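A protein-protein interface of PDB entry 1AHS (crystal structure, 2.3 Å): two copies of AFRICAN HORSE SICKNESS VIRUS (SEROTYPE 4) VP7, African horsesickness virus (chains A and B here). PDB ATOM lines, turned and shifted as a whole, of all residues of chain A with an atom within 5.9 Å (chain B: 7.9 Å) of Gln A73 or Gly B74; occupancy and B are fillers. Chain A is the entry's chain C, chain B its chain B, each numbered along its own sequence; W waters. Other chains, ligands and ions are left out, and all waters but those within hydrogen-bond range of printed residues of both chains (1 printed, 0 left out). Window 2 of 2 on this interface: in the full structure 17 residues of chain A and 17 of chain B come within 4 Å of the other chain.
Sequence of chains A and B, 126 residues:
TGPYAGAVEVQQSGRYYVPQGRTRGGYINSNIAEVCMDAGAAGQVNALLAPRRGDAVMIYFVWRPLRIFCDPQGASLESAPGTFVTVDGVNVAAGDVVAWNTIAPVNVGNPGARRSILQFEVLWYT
The backbone NH (N) of Ser B76 sits at hydrogen-bond distance from the backbone carbonyl oxygen (O) of Pro A72.
The backbone NH (N) of Gly A74 lies within hydrogen-bond range of the backbone carbonyl oxygen (O) of Gly B74, at 3.1 Å.
The backbone carbonyl oxygen of Gly B74 sits at hydrogen-bond distance from the guanidinium group of Arg A15 (2.6 Å).
NH2 of Arg A15 lies close to SG of Cys B70, at 3.6 Å.
The guanidinium group of Arg A15 sits at hydrogen-bond distance from the side-chain hydroxyl of Ser B76 (3.1 Å).
O of Pro A72 is in hydrogen-bond range of NH1 of Arg A15.
OD1 of Asp A71 sits at hydrogen-bond distance from N of Gln A73, 2.9 Å away.
SG of Cys A70 sits at hydrogen-bond distance from NH2 of Arg A15 (3.6 Å).
The side-chain carboxylate (OD1) of Asp B71 lies within hydrogen-bond range of the backbone NH (N) of Gly B74 (3.2 Å).
OD1 of Asp B71 lies within hydrogen-bond range of N of Ala B75 (3.3 Å).
The backbone NH (N) of Gly A74 sits at hydrogen-bond distance from the side-chain carboxylate (OD1) of Asp A71 (3.0 Å).
Among the printed residues, pairs that only touch across the chains: Gln A73 with Gly B74 (3.3 Å), Arg A15 with Ala B75 (3.6 Å), Pro A72 with Ala B75 (3.7 Å) and Pro A72 with Gly B74 (3.8 Å).
Of the printed residues of chain B, Arg A15 touches Cys B70 (3.3 Å), Gly B74 (2.6 Å), Ala B75 (3.6 Å) and Ser B76 (3.1 Å).
Cys A70 touches none of the printed residues of chain B.
Printed residues of chain B within 4 Å of Pro A72: Gly B74 (3.8 Å), Ala B75 (3.7 Å) and Ser B76 (3.0 Å).
Gln A73 touches one residue of chain B.
Phe B69 touches none of the printed residues of chain A.
Printed residues of chain A within 4 Å of Cys B70: Arg A15.
Gly B74 touches just these residues of chain A: Arg A15 (2.6 Å), Pro A72 (3.8 Å), Gln A73 (3.3 Å) and Gly A74 (3.1 Å).
Printed residues of chain A within 4 Å of Ala B75: Arg A15 and Pro A72.
Of the printed residues of chain A, Ser B76 touches Arg A15 and Pro A72.
The nearest residue of chain A that does not touch Gly B74 is Asp A71 (4.7 Å).
The nearest printed residue of chain A that does not touch Cys B70 is Pro A72 (6.5 Å).
Of the 7 printed residues of chain A, 4 touch a printed residue of chain B.
Hydrophobic or aromatic side chains of chain A that line the printed part of chain B: Pro A72.
Along chain A the printed residues that touch a printed residue of chain B span positions 15 to 74.
Printed residues of chain B that touch a printed residue of chain A: Cys B70, Gly B74, Ala B75 and Ser B76.
Arg A15 touches Gly B74, but with the chains exchanged Gly A74 does not touch Arg B15 (5.8 Å).
Arg A15 touches Ala B75, but with the chains exchanged Ala A75 does not touch Arg B15 (7.8 Å).
Pro A72 touches Gly B74, but with the chains exchanged Gly A74 does not touch Pro B72 (8.9 Å).
Pro A72 touches Ala B75, but with the chains exchanged Ala A75 does not touch Pro B72 (10.7 Å).
Positions printed for both chains: 15, 70, 71, 72, 73, 74 and 75.
Water W1 lies within hydrogen-bond range of NH2 of Arg A15 (3.1 Å) and NH2 of Arg B15 (3.3 Å).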
ATOM      1  N   ARG A  15      34.227  22.319 -20.717  1.00  0.00           N
ATOM      2  CA  ARG A  15      32.782  22.425 -20.895  1.00  0.00           C
ATOM      3  C   ARG A  15      32.402  23.799 -20.456  1.00  0.00           C
ATOM      4  O   ARG A  15      32.416  24.096 -19.290  1.00  0.00           O
ATOM      5  CB  ARG A  15      32.031  21.382 -20.060  1.00  0.00           C
ATOM      6  CG  ARG A  15      30.555  21.535 -20.079  1.00  0.00           C
ATOM      7  CD  ARG A  15      29.844  20.243 -19.741  1.00  0.00           C
ATOM      8  NE  ARG A  15      30.041  19.249 -20.764  1.00  0.00           N
ATOM      9  CZ  ARG A  15      29.144  18.949 -21.695  1.00  0.00           C
ATOM     10  NH1 ARG A  15      27.982  19.564 -21.719  1.00  0.00           N
ATOM     11  NH2 ARG A  15      29.414  18.040 -22.612  1.00  0.00           N
ATOM     12  N   CYS A  70      33.679  22.503 -25.673  1.00  0.00           N
ATOM     13  CA  CYS A  70      32.267  22.346 -26.017  1.00  0.00           C
ATOM     14  C   CYS A  70      31.332  23.371 -25.352  1.00  0.00           C
ATOM     15  O   CYS A  70      31.688  24.057 -24.381  1.00  0.00           O
ATOM     16  CB  CYS A  70      31.790  20.934 -25.672  1.00  0.00           C
ATOM     17  SG  CYS A  70      31.538  20.551 -23.997  1.00  0.00           S
ATOM     18  N   ASP A  71      30.154  23.541 -25.920  1.00  0.00           N
ATOM     19  CA  ASP A  71      29.195  24.435 -25.334  1.00  0.00           C
ATOM     20  C   ASP A  71      28.355  23.570 -24.396  1.00  0.00           C
ATOM     21  O   ASP A  71      28.502  22.346 -24.361  1.00  0.00           O
ATOM     22  CB  ASP A  71      28.372  25.147 -26.422  1.00  0.00           C
ATOM     23  CG  ASP A  71      27.426  24.225 -27.190  1.00  0.00           C
ATOM     24  OD1 ASP A  71      27.265  23.056 -26.845  1.00  0.00           O
ATOM     25  OD2 ASP A  71      26.788  24.688 -28.144  1.00  0.00           O
ATOM     26  N   PRO A  72      27.404  24.174 -23.685  1.00  0.00           N
ATOM     27  CA  PRO A  72      26.582  23.398 -22.756  1.00  0.00           C
ATOM     28  C   PRO A  72      25.787  22.249 -23.310  1.00  0.00           C
ATOM     29  O   PRO A  72      25.346  21.408 -22.542  1.00  0.00           O
ATOM     30  CB  PRO A  72      25.675  24.449 -22.153  1.00  0.00           C
ATOM     31  CG  PRO A  72      26.526  25.698 -22.216  1.00  0.00           C
ATOM     32  CD  PRO A  72      27.091  25.610 -23.590  1.00  0.00           C
ATOM     33  N   GLN A  73      25.532  22.213 -24.614  1.00  0.00           N
ATOM     34  CA  GLN A  73      24.764  21.092 -25.170  1.00  0.00           C
ATOM     35  C   GLN A  73      25.686  20.102 -25.842  1.00  0.00           C
ATOM     36  O   GLN A  73      25.251  19.243 -26.593  1.00  0.00           O
ATOM     37  CB  GLN A  73      23.655  21.520 -26.128  1.00  0.00           C
ATOM     38  CG  GLN A  73      22.923  22.770 -25.751  1.00  0.00           C
ATOM     39  CD  GLN A  73      23.394  23.931 -26.612  1.00  0.00           C
ATOM     40  OE1 GLN A  73      23.184  23.924 -27.837  1.00  0.00           O
ATOM     41  NE2 GLN A  73      24.057  24.928 -25.996  1.00  0.00           N
ATOM     42  N   GLY A  74      26.981  20.292 -25.632  1.00  0.00           N
ATOM     43  CA  GLY A  74      27.926  19.352 -26.148  1.00  0.00           C
ATOM     44  C   GLY A  74      28.508  19.488 -27.518  1.00  0.00           C
ATOM     45  O   GLY A  74      29.290  18.610 -27.900  1.00  0.00           O
ATOM     46  N   ALA A  75      28.241  20.584 -28.217  1.00  0.00           N
ATOM     47  CA  ALA A  75      28.794  20.810 -29.559  1.00  0.00           C
ATOM     48  C   ALA A  75      30.180  21.404 -29.500  1.00  0.00           C
ATOM     49  O   ALA A  75      30.464  22.163 -28.596  1.00  0.00           O
ATOM     50  CB  ALA A  75      27.882  21.726 -30.351  1.00  0.00           C
ATOM     51  N   GLN B  12      36.982   9.470 -20.828  1.00  0.00           N
ATOM     52  CA  GLN B  12      36.955  10.912 -20.796  1.00  0.00           C
ATOM     53  C   GLN B  12      36.416  11.299 -19.484  1.00  0.00           C
ATOM     54  O   GLN B  12      35.413  10.781 -19.038  1.00  0.00           O
ATOM     55  CB  GLN B  12      36.054  11.480 -21.888  1.00  0.00           C
ATOM     56  CG  GLN B  12      35.922  12.991 -21.835  1.00  0.00           C
ATOM     57  CD  GLN B  12      34.893  13.549 -22.784  1.00  0.00           C
ATOM     58  OE1 GLN B  12      33.816  12.994 -22.966  1.00  0.00           O
ATOM     59  NE2 GLN B  12      35.198  14.697 -23.346  1.00  0.00           N
ATOM     60  N   ARG B  15      32.237  12.401 -18.199  1.00  0.00           N
ATOM     61  CA  ARG B  15      31.166  11.901 -19.041  1.00  0.00           C
ATOM     62  C   ARG B  15      30.456  10.736 -18.341  1.00  0.00           C
ATOM     63  O   ARG B  15      31.044   9.681 -18.124  1.00  0.00           O
ATOM     64  CB  ARG B  15      31.703  11.465 -20.404  1.00  0.00           C
ATOM     65  CG  ARG B  15      30.599  10.904 -21.335  1.00  0.00           C
ATOM     66  CD  ARG B  15      31.050  10.856 -22.782  1.00  0.00           C
ATOM     67  NE  ARG B  15      31.049  12.182 -23.363  1.00  0.00           N
ATOM     68  CZ  ARG B  15      30.031  12.680 -24.055  1.00  0.00           C
ATOM     69  NH1 ARG B  15      28.943  11.944 -24.244  1.00  0.00           N
ATOM     70  NH2 ARG B  15      30.115  13.909 -24.571  1.00  0.00           N
ATOM     71  N   PHE B  69      29.098  18.307 -15.327  1.00  0.00           N
ATOM     72  CA  PHE B  69      29.601  17.193 -16.095  1.00  0.00           C
ATOM     73  C   PHE B  69      28.561  16.955 -17.197  1.00  0.00           C
ATOM     74  O   PHE B  69      27.712  17.799 -17.371  1.00  0.00           O
ATOM     75  CB  PHE B  69      29.851  15.976 -15.178  1.00  0.00           C
ATOM     76  CG  PHE B  69      28.614  15.382 -14.566  1.00  0.00           C
ATOM     77  CD1 PHE B  69      28.156  15.817 -13.346  1.00  0.00           C
ATOM     78  CD2 PHE B  69      27.948  14.352 -15.192  1.00  0.00           C
ATOM     79  CE1 PHE B  69      27.048  15.227 -12.762  1.00  0.00           C
ATOM     80  CE2 PHE B  69      26.853  13.761 -14.617  1.00  0.00           C
ATOM     81  CZ  PHE B  69      26.411  14.210 -13.395  1.00  0.00           C
ATOM     82  N   CYS B  70      28.577  15.849 -17.933  1.00  0.00           N
ATOM     83  CA  CYS B  70      27.561  15.660 -18.978  1.00  0.00           C
ATOM     84  C   CYS B  70      26.918  14.283 -19.011  1.00  0.00           C
ATOM     85  O   CYS B  70      27.414  13.325 -18.421  1.00  0.00           O
ATOM     86  CB  CYS B  70      28.133  15.976 -20.357  1.00  0.00           C
ATOM     87  SG  CYS B  70      29.364  14.883 -20.951  1.00  0.00           S
ATOM     88  N   ASP B  71      25.749  14.209 -19.622  1.00  0.00           N
ATOM     89  CA  ASP B  71      25.070  12.932 -19.767  1.00  0.00           C
ATOM     90  C   ASP B  71      25.616  12.256 -21.022  1.00  0.00           C
ATOM     91  O   ASP B  71      26.475  12.800 -21.691  1.00  0.00           O
ATOM     92  CB  ASP B  71      23.518  13.077 -19.751  1.00  0.00           C
ATOM     93  CG  ASP B  71      22.930  13.777 -20.979  1.00  0.00           C
ATOM     94  OD1 ASP B  71      23.617  13.994 -21.995  1.00  0.00           O
ATOM     95  OD2 ASP B  71      21.719  14.084 -20.915  1.00  0.00           O
ATOM     96  N   PRO B  72      25.140  11.059 -21.355  1.00  0.00           N
ATOM     97  CA  PRO B  72      25.655  10.397 -22.537  1.00  0.00           C
ATOM     98  C   PRO B  72      25.421  11.077 -23.858  1.00  0.00           C
ATOM     99  O   PRO B  72      26.050  10.693 -24.837  1.00  0.00           O
ATOM    100  CB  PRO B  72      24.971   9.070 -22.478  1.00  0.00           C
ATOM    101  CG  PRO B  72      24.925   8.824 -21.026  1.00  0.00           C
ATOM    102  CD  PRO B  72      24.353  10.117 -20.559  1.00  0.00           C
ATOM    103  N   GLN B  73      24.575  12.110 -23.873  1.00  0.00           N
ATOM    104  CA  GLN B  73      24.263  12.879 -25.075  1.00  0.00           C
ATOM    105  C   GLN B  73      25.038  14.177 -25.252  1.00  0.00           C
ATOM    106  O   GLN B  73      24.845  14.863 -26.274  1.00  0.00           O
ATOM    107  CB  GLN B  73      22.783  13.227 -25.143  1.00  0.00           C
ATOM    108  CG  GLN B  73      21.912  12.193 -25.824  1.00  0.00           C
ATOM    109  CD  GLN B  73      21.500  11.095 -24.876  1.00  0.00           C
ATOM    110  OE1 GLN B  73      21.478   9.908 -25.248  1.00  0.00           O
ATOM    111  NE2 GLN B  73      21.182  11.477 -23.623  1.00  0.00           N
ATOM    112  N   GLY B  74      25.790  14.587 -24.223  1.00  0.00           N
ATOM    113  CA  GLY B  74      26.625  15.790 -24.305  1.00  0.00           C
ATOM    114  C   GLY B  74      26.126  17.012 -23.577  1.00  0.00           C
ATOM    115  O   GLY B  74      26.827  18.029 -23.486  1.00  0.00           O
ATOM    116  N   ALA B  75      24.958  16.859 -22.967  1.00  0.00           N
ATOM    117  CA  ALA B  75      24.261  17.905 -22.217  1.00  0.00           C
ATOM    118  C   ALA B  75      24.783  18.111 -20.804  1.00  0.00           C
ATOM    119  O   ALA B  75      25.045  17.135 -20.115  1.00  0.00           O
ATOM    120  CB  ALA B  75      22.821  17.529 -22.142  1.00  0.00           C
ATOM    121  N   SER B  76      24.906  19.362 -20.362  1.00  0.00           N
ATOM    122  CA  SER B  76      25.406  19.643 -19.025  1.00  0.00           C
ATOM    123  C   SER B  76      24.501  19.174 -17.908  1.00  0.00           C
ATOM    124  O   SER B  76      23.296  19.390 -17.921  1.00  0.00           O
ATOM    125  CB  SER B  76      25.693  21.119 -18.845  1.00  0.00           C
ATOM    126  OG  SER B  76      26.722  21.532 -19.713  1.00  0.00           O
ATOM    127  N   LEU B  77      25.116  18.666 -16.862  1.00  0.00           N
ATOM    128  CA  LEU B  77      24.397  18.135 -15.727  1.00  0.00           C
ATOM    129  C   LEU B  77      25.198  18.608 -14.503  1.00  0.00           C
ATOM    130  O   LEU B  77      26.376  18.958 -14.659  1.00  0.00           O
ATOM    131  CB  LEU B  77      24.482  16.632 -15.872  1.00  0.00           C
ATOM    132  CG  LEU B  77      23.274  15.732 -15.767  1.00  0.00           C
ATOM    133  CD1 LEU B  77      22.184  16.306 -16.590  1.00  0.00           C
ATOM    134  CD2 LEU B  77      23.642  14.325 -16.210  1.00  0.00           C
HETATM  135  O   HOH W   1      31.906  16.491 -23.458  1.00  0.00           O
